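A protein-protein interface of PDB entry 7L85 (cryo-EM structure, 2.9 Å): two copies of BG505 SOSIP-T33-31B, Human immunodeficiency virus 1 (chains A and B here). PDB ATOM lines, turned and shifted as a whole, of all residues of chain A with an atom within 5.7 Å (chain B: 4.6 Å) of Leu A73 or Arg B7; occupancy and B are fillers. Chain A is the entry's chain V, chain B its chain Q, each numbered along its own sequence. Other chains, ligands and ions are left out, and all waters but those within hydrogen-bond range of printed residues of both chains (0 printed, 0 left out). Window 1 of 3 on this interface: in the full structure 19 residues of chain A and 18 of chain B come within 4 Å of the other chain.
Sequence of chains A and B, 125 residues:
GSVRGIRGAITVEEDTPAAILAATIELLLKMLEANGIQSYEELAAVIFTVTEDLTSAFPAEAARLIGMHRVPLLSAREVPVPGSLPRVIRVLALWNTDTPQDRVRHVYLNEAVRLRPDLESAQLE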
ATOM      1  N   VAL A  46      -0.206  -4.787 -22.326  1.00  0.00           N
ATOM      2  CA  VAL A  46       0.047  -3.387 -22.006  1.00  0.00           C
ATOM      3  C   VAL A  46       0.287  -2.554 -23.253  1.00  0.00           C
ATOM      4  O   VAL A  46       1.123  -2.907 -24.084  1.00  0.00           O
ATOM      5  CB  VAL A  46       1.231  -3.247 -21.064  1.00  0.00           C
ATOM      6  CG1 VAL A  46       1.500  -1.804 -20.768  1.00  0.00           C
ATOM      7  CG2 VAL A  46       0.937  -3.964 -19.813  1.00  0.00           C
ATOM      8  N   PHE A  48       1.438   1.152 -24.689  1.00  0.00           N
ATOM      9  CA  PHE A  48       2.092   2.401 -24.342  1.00  0.00           C
ATOM     10  C   PHE A  48       1.913   3.411 -25.428  1.00  0.00           C
ATOM     11  O   PHE A  48       2.087   3.077 -26.596  1.00  0.00           O
ATOM     12  CB  PHE A  48       3.593   2.202 -24.251  1.00  0.00           C
ATOM     13  CG  PHE A  48       4.053   1.314 -23.228  1.00  0.00           C
ATOM     14  CD1 PHE A  48       4.110  -0.009 -23.470  1.00  0.00           C
ATOM     15  CD2 PHE A  48       4.471   1.772 -22.043  1.00  0.00           C
ATOM     16  CE1 PHE A  48       4.555  -0.852 -22.542  1.00  0.00           C
ATOM     17  CE2 PHE A  48       4.921   0.924 -21.101  1.00  0.00           C
ATOM     18  CZ  PHE A  48       4.960  -0.394 -21.352  1.00  0.00           C
ATOM     19  N   ALA A  60       8.351   0.457 -23.947  1.00  0.00           N
ATOM     20  CA  ALA A  60       8.171  -0.967 -23.828  1.00  0.00           C
ATOM     21  C   ALA A  60       9.446  -1.657 -23.391  1.00  0.00           C
ATOM     22  O   ALA A  60       9.396  -2.722 -22.791  1.00  0.00           O
ATOM     23  CB  ALA A  60       7.700  -1.531 -25.138  1.00  0.00           C
ATOM     24  N   GLU A  61      10.606  -1.101 -23.703  1.00  0.00           N
ATOM     25  CA  GLU A  61      11.839  -1.734 -23.302  1.00  0.00           C
ATOM     26  C   GLU A  61      11.961  -1.740 -21.798  1.00  0.00           C
ATOM     27  O   GLU A  61      12.493  -2.677 -21.216  1.00  0.00           O
ATOM     28  CB  GLU A  61      13.024  -1.038 -23.934  1.00  0.00           C
ATOM     29  CG  GLU A  61      13.131  -1.277 -25.419  1.00  0.00           C
ATOM     30  CD  GLU A  61      14.180  -0.433 -26.118  1.00  0.00           C
ATOM     31  OE1 GLU A  61      14.482   0.643 -25.647  1.00  0.00           O
ATOM     32  OE2 GLU A  61      14.674  -0.872 -27.134  1.00  0.00           O
ATOM     33  N   ALA A  63       9.701  -2.073 -19.677  1.00  0.00           N
ATOM     34  CA  ALA A  63       8.873  -3.118 -19.132  1.00  0.00           C
ATOM     35  C   ALA A  63       9.650  -4.413 -18.969  1.00  0.00           C
ATOM     36  O   ALA A  63       9.352  -5.204 -18.073  1.00  0.00           O
ATOM     37  CB  ALA A  63       7.684  -3.340 -20.002  1.00  0.00           C
ATOM     38  N   ARG A  64      10.667  -4.658 -19.786  1.00  0.00           N
ATOM     39  CA  ARG A  64      11.388  -5.898 -19.657  1.00  0.00           C
ATOM     40  C   ARG A  64      12.505  -5.789 -18.641  1.00  0.00           C
ATOM     41  O   ARG A  64      13.144  -6.782 -18.305  1.00  0.00           O
ATOM     42  CB  ARG A  64      11.939  -6.325 -20.976  1.00  0.00           C
ATOM     43  CG  ARG A  64      10.894  -6.721 -21.967  1.00  0.00           C
ATOM     44  CD  ARG A  64      11.517  -7.172 -23.204  1.00  0.00           C
ATOM     45  NE  ARG A  64      12.306  -8.414 -22.997  1.00  0.00           N
ATOM     46  CZ  ARG A  64      13.295  -8.847 -23.816  1.00  0.00           C
ATOM     47  NH1 ARG A  64      13.634  -8.146 -24.891  1.00  0.00           N
ATOM     48  NH2 ARG A  64      13.931  -9.975 -23.539  1.00  0.00           N
ATOM     49  N   MET A  68       8.632  -7.938 -17.184  1.00  0.00           N
ATOM     50  CA  MET A  68       7.400  -8.280 -17.870  1.00  0.00           C
ATOM     51  C   MET A  68       7.705  -8.918 -19.203  1.00  0.00           C
ATOM     52  O   MET A  68       7.250  -8.470 -20.245  1.00  0.00           O
ATOM     53  CB  MET A  68       6.603  -7.014 -18.055  1.00  0.00           C
ATOM     54  CG  MET A  68       6.164  -6.429 -16.775  1.00  0.00           C
ATOM     55  SD  MET A  68       5.464  -4.851 -16.912  1.00  0.00           S
ATOM     56  CE  MET A  68       3.958  -5.147 -17.658  1.00  0.00           C
ATOM     57  N   VAL A  71       4.527 -10.412 -20.974  1.00  0.00           N
ATOM     58  CA  VAL A  71       3.344  -9.611 -21.108  1.00  0.00           C
ATOM     59  C   VAL A  71       3.390  -9.020 -22.487  1.00  0.00           C
ATOM     60  O   VAL A  71       4.408  -8.455 -22.835  1.00  0.00           O
ATOM     61  CB  VAL A  71       3.327  -8.487 -20.098  1.00  0.00           C
ATOM     62  CG1 VAL A  71       2.084  -7.652 -20.271  1.00  0.00           C
ATOM     63  CG2 VAL A  71       3.398  -9.048 -18.742  1.00  0.00           C
ATOM     64  N   PRO A  72       2.399  -9.188 -23.346  1.00  0.00           N
ATOM     65  CA  PRO A  72       2.389  -8.606 -24.656  1.00  0.00           C
ATOM     66  C   PRO A  72       2.522  -7.107 -24.548  1.00  0.00           C
ATOM     67  O   PRO A  72       1.710  -6.477 -23.873  1.00  0.00           O
ATOM     68  CB  PRO A  72       1.007  -9.001 -25.129  1.00  0.00           C
ATOM     69  CG  PRO A  72       0.701 -10.216 -24.368  1.00  0.00           C
ATOM     70  CD  PRO A  72       1.285 -10.017 -23.048  1.00  0.00           C
ATOM     71  N   LEU A  73       3.458  -6.514 -25.270  1.00  0.00           N
ATOM     72  CA  LEU A  73       3.621  -5.073 -25.187  1.00  0.00           C
ATOM     73  C   LEU A  73       3.505  -4.454 -26.551  1.00  0.00           C
ATOM     74  O   LEU A  73       4.207  -4.861 -27.483  1.00  0.00           O
ATOM     75  CB  LEU A  73       4.987  -4.711 -24.640  1.00  0.00           C
ATOM     76  CG  LEU A  73       5.393  -5.334 -23.332  1.00  0.00           C
ATOM     77  CD1 LEU A  73       6.773  -4.922 -23.044  1.00  0.00           C
ATOM     78  CD2 LEU A  73       4.468  -4.969 -22.205  1.00  0.00           C
ATOM     79  N   LEU A  74       2.629  -3.484 -26.673  1.00  0.00           N
ATOM     80  CA  LEU A  74       2.412  -2.795 -27.932  1.00  0.00           C
ATOM     81  C   LEU A  74       2.604  -1.310 -27.721  1.00  0.00           C
ATOM     82  O   LEU A  74       2.289  -0.817 -26.642  1.00  0.00           O
ATOM     83  CB  LEU A  74       0.996  -3.049 -28.422  1.00  0.00           C
ATOM     84  CG  LEU A  74       0.631  -2.594 -29.835  1.00  0.00           C
ATOM     85  CD1 LEU A  74       1.323  -3.502 -30.859  1.00  0.00           C
ATOM     86  CD2 LEU A  74      -0.849  -2.622 -29.992  1.00  0.00           C
ATOM     87  N   SER A  75       3.094  -0.575 -28.707  1.00  0.00           N
ATOM     88  CA  SER A  75       3.175   0.860 -28.513  1.00  0.00           C
ATOM     89  C   SER A  75       2.736   1.643 -29.732  1.00  0.00           C
ATOM     90  O   SER A  75       2.771   1.154 -30.854  1.00  0.00           O
ATOM     91  CB  SER A  75       4.578   1.245 -28.134  1.00  0.00           C
ATOM     92  OG  SER A  75       5.471   0.961 -29.161  1.00  0.00           O
ATOM     93  N   GLY B   5      -3.148 -11.515 -24.506  1.00  0.00           N
ATOM     94  CA  GLY B   5      -2.751 -10.953 -25.762  1.00  0.00           C
ATOM     95  C   GLY B   5      -1.808 -11.897 -26.482  1.00  0.00           C
ATOM     96  O   GLY B   5      -1.053 -12.630 -25.847  1.00  0.00           O
ATOM     97  N   ILE B   6      -1.810 -11.838 -27.797  1.00  0.00           N
ATOM     98  CA  ILE B   6      -0.908 -12.609 -28.623  1.00  0.00           C
ATOM     99  C   ILE B   6      -0.131 -11.624 -29.441  1.00  0.00           C
ATOM    100  O   ILE B   6      -0.721 -10.773 -30.092  1.00  0.00           O
ATOM    101  CB  ILE B   6      -1.637 -13.506 -29.617  1.00  0.00           C
ATOM    102  CG1 ILE B   6      -2.580 -14.428 -28.926  1.00  0.00           C
ATOM    103  CG2 ILE B   6      -0.591 -14.335 -30.356  1.00  0.00           C
ATOM    104  CD1 ILE B   6      -3.527 -15.126 -29.858  1.00  0.00           C
ATOM    105  N   ARG B   7       1.175 -11.714 -29.467  1.00  0.00           N
ATOM    106  CA  ARG B   7       1.922 -10.772 -30.259  1.00  0.00           C
ATOM    107  C   ARG B   7       2.718 -11.390 -31.348  1.00  0.00           C
ATOM    108  O   ARG B   7       3.229 -12.502 -31.225  1.00  0.00           O
ATOM    109  CB  ARG B   7       2.875  -9.981 -29.393  1.00  0.00           C
ATOM    110  CG  ARG B   7       2.250  -8.862 -28.663  1.00  0.00           C
ATOM    111  CD  ARG B   7       2.220  -7.579 -29.429  1.00  0.00           C
ATOM    112  NE  ARG B   7       3.465  -6.871 -29.351  1.00  0.00           N
ATOM    113  CZ  ARG B   7       4.449  -6.848 -30.239  1.00  0.00           C
ATOM    114  NH1 ARG B   7       4.390  -7.512 -31.355  1.00  0.00           N
ATOM    115  NH2 ARG B   7       5.485  -6.127 -29.919  1.00  0.00           N
ATOM    116  N   GLY B   8       2.905 -10.618 -32.383  1.00  0.00           N
ATOM    117  CA  GLY B   8       3.834 -11.028 -33.388  1.00  0.00           C
ATOM    118  C   GLY B   8       4.244  -9.899 -34.282  1.00  0.00           C
ATOM    119  O   GLY B   8       3.687  -8.802 -34.228  1.00  0.00           O
ATOM    120  N   MET B  31       0.279 -16.727 -36.395  1.00  0.00           N
ATOM    121  CA  MET B  31      -0.076 -16.528 -34.994  1.00  0.00           C
ATOM    122  C   MET B  31      -1.213 -17.427 -34.596  1.00  0.00           C
ATOM    123  O   MET B  31      -1.183 -18.068 -33.540  1.00  0.00           O
ATOM    124  CB  MET B  31      -0.490 -15.086 -34.747  1.00  0.00           C
ATOM    125  CG  MET B  31       0.611 -14.086 -34.818  1.00  0.00           C
ATOM    126  SD  MET B  31       0.026 -12.386 -34.822  1.00  0.00           S
ATOM    127  CE  MET B  31      -0.548 -12.056 -33.184  1.00  0.00           C
ATOM    128  N   ARG B  90       3.460  -4.927 -36.788  1.00  0.00           N
ATOM    129  CA  ARG B  90       3.292  -5.606 -35.511  1.00  0.00           C
ATOM    130  C   ARG B  90       1.840  -5.838 -35.224  1.00  0.00           C
ATOM    131  O   ARG B  90       0.997  -4.993 -35.506  1.00  0.00           O
ATOM    132  CB  ARG B  90       3.857  -4.810 -34.371  1.00  0.00           C
ATOM    133  CG  ARG B  90       5.322  -4.630 -34.361  1.00  0.00           C
ATOM    134  CD  ARG B  90       5.727  -3.866 -33.190  1.00  0.00           C
ATOM    135  NE  ARG B  90       7.168  -3.824 -32.978  1.00  0.00           N
ATOM    136  CZ  ARG B  90       8.012  -2.993 -33.594  1.00  0.00           C
ATOM    137  NH1 ARG B  90       7.575  -2.205 -34.498  1.00  0.00           N
ATOM    138  NH2 ARG B  90       9.277  -2.975 -33.259  1.00  0.00           N
ATOM    139  N   VAL B  91       1.530  -6.978 -34.653  1.00  0.00           N
ATOM    140  CA  VAL B  91       0.159  -7.273 -34.329  1.00  0.00           C
ATOM    141  C   VAL B  91      -0.051  -7.723 -32.914  1.00  0.00           C
ATOM    142  O   VAL B  91       0.670  -8.586 -32.419  1.00  0.00           O
ATOM    143  CB  VAL B  91      -0.368  -8.373 -35.251  1.00  0.00           C
ATOM    144  CG1 VAL B  91      -1.796  -8.689 -34.929  1.00  0.00           C
ATOM    145  CG2 VAL B  91      -0.260  -7.933 -36.638  1.00  0.00           C
ATOM    146  N   LEU B  92      -1.053  -7.146 -32.262  1.00  0.00           N
ATOM    147  CA  LEU B  92      -1.505  -7.583 -30.953  1.00  0.00           C
ATOM    148  C   LEU B  92      -2.909  -8.117 -31.047  1.00  0.00           C
ATOM    149  O   LEU B  92      -3.828  -7.380 -31.392  1.00  0.00           O
ATOM    150  CB  LEU B  92      -1.542  -6.444 -29.945  1.00  0.00           C
ATOM    151  CG  LEU B  92      -2.169  -6.767 -28.553  1.00  0.00           C
ATOM    152  CD1 LEU B  92      -1.377  -7.793 -27.815  1.00  0.00           C
ATOM    153  CD2 LEU B  92      -2.246  -5.507 -27.755  1.00  0.00           C
ATOM    154  N   HIS B 106       4.146 -16.555 -29.305  1.00  0.00           N
ATOM    155  CA  HIS B 106       4.255 -15.320 -30.045  1.00  0.00           C
ATOM    156  C   HIS B 106       5.034 -15.583 -31.301  1.00  0.00           C
ATOM    157  O   HIS B 106       5.840 -16.510 -31.349  1.00  0.00           O
ATOM    158  CB  HIS B 106       4.917 -14.292 -29.163  1.00  0.00           C
ATOM    159  CG  HIS B 106       4.146 -14.087 -27.914  1.00  0.00           C
ATOM    160  ND1 HIS B 106       3.005 -13.341 -27.852  1.00  0.00           N
ATOM    161  CD2 HIS B 106       4.347 -14.560 -26.682  1.00  0.00           C
ATOM    162  CE1 HIS B 106       2.542 -13.370 -26.624  1.00  0.00           C
ATOM    163  NE2 HIS B 106       3.338 -14.100 -25.902  1.00  0.00           N
ATOM    164  N   VAL B 107       4.766 -14.816 -32.338  1.00  0.00           N
ATOM    165  CA  VAL B 107       5.410 -15.066 -33.616  1.00  0.00           C
ATOM    166  C   VAL B 107       6.224 -13.945 -34.200  1.00  0.00           C
ATOM    167  O   VAL B 107       5.700 -12.872 -34.446  1.00  0.00           O
ATOM    168  CB  VAL B 107       4.323 -15.438 -34.622  1.00  0.00           C
ATOM    169  CG1 VAL B 107       4.880 -15.638 -35.948  1.00  0.00           C
ATOM    170  CG2 VAL B 107       3.656 -16.690 -34.190  1.00  0.00           C
ATOM    171  N   TYR B 108       7.480 -14.213 -34.475  1.00  0.00           N
ATOM    172  CA  TYR B 108       8.338 -13.215 -35.077  1.00  0.00           C
ATOM    173  C   TYR B 108       8.911 -13.765 -36.349  1.00  0.00           C
ATOM    174  O   TYR B 108       9.551 -14.810 -36.346  1.00  0.00           O
ATOM    175  CB  TYR B 108       9.405 -12.810 -34.103  1.00  0.00           C
ATOM    176  CG  TYR B 108       8.828 -12.177 -32.922  1.00  0.00           C
ATOM    177  CD1 TYR B 108       8.390 -12.916 -31.881  1.00  0.00           C
ATOM    178  CD2 TYR B 108       8.721 -10.857 -32.885  1.00  0.00           C
ATOM    179  CE1 TYR B 108       7.842 -12.311 -30.809  1.00  0.00           C
ATOM    180  CE2 TYR B 108       8.173 -10.245 -31.814  1.00  0.00           C
ATOM    181  CZ  TYR B 108       7.737 -10.970 -30.785  1.00  0.00           C
ATOM    182  OH  TYR B 108       7.193 -10.352 -29.705  1.00  0.00           O
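O of Leu A73 sits at hydrogen-bond distance from NE of Arg B7, at 2.8 Å.
A ring nitrogen (ND1) of His B106 sits at hydrogen-bond distance from the backbone NH of Arg B7 (2.9 Å).
N of Phe A48 sits at hydrogen-bond distance from O of Leu A74.
The backbone carbonyl oxygen (O) of Pro A72 is in hydrogen-bond range of the backbone NH (N) of Val A46 (3.0 Å).
The backbone carbonyl oxygen of Arg B7 is in hydrogen-bond range of the backbone NH of Val B107 (3.0 Å).
The backbone NH (N) of Leu A74 lies within hydrogen-bond range of the backbone carbonyl oxygen (O) of Val A46 (3.1 Å).
CG of Pro A72 touches O of Gly B5, 3.3 Å away.
CG of Arg B7 touches CB of Pro A72, at 3.7 Å.
CB of Pro A72 touches CD1 of Leu B92, at 3.8 Å.
CB of Leu B92 touches CD2 of Leu A74, at 3.9 Å.
Of chain B, only Arg B7 comes within 4 Å of Leu A73.
Of chain A, only Pro A72 (3.7 Å) and Leu A73 (2.8 Å) come within 4 Å of Arg B7.
Printed residues of chain A within 4 Å of Gly B5: Pro A72 (3.3 Å).
Of the printed residues of chain A, Leu B92 touches Pro A72 (3.8 Å) and Leu A74 (3.9 Å).
Printed residues of chain B within 4 Å of Leu A74: Leu B92 (3.9 Å).
Printed residues of chain B within 4 Å of Pro A72: Gly B5 (3.3 Å), Arg B7 (3.7 Å) and Leu B92 (3.8 Å).
Ser A75 touches none of the printed residues of chain B.
Glu A61 touches none of the printed residues of chain B.
The nearest printed residue of chain B that does not touch Leu A73 is Leu B92 (5.6 Å).
Hydrophobic or aromatic side chains of chain A within 4 Å of the printed part of chain B: Pro A72 and Leu A74.
Printed residues of chain B that touch a printed residue of chain A: Gly B5, Arg B7 and Leu B92.
Hydrophobic or aromatic side chains of chain B within 4 Å of the printed part of chain A: Leu B92.
Among the printed residues, no Asp or Glu carboxylate lies within 4 Å of a Lys or Arg side-chain nitrogen of the other chain.
No position is printed for both chains.
Of the 5 pairs that touch across the chains among the printed residues, none has its exchanged pair printed and touching as well.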
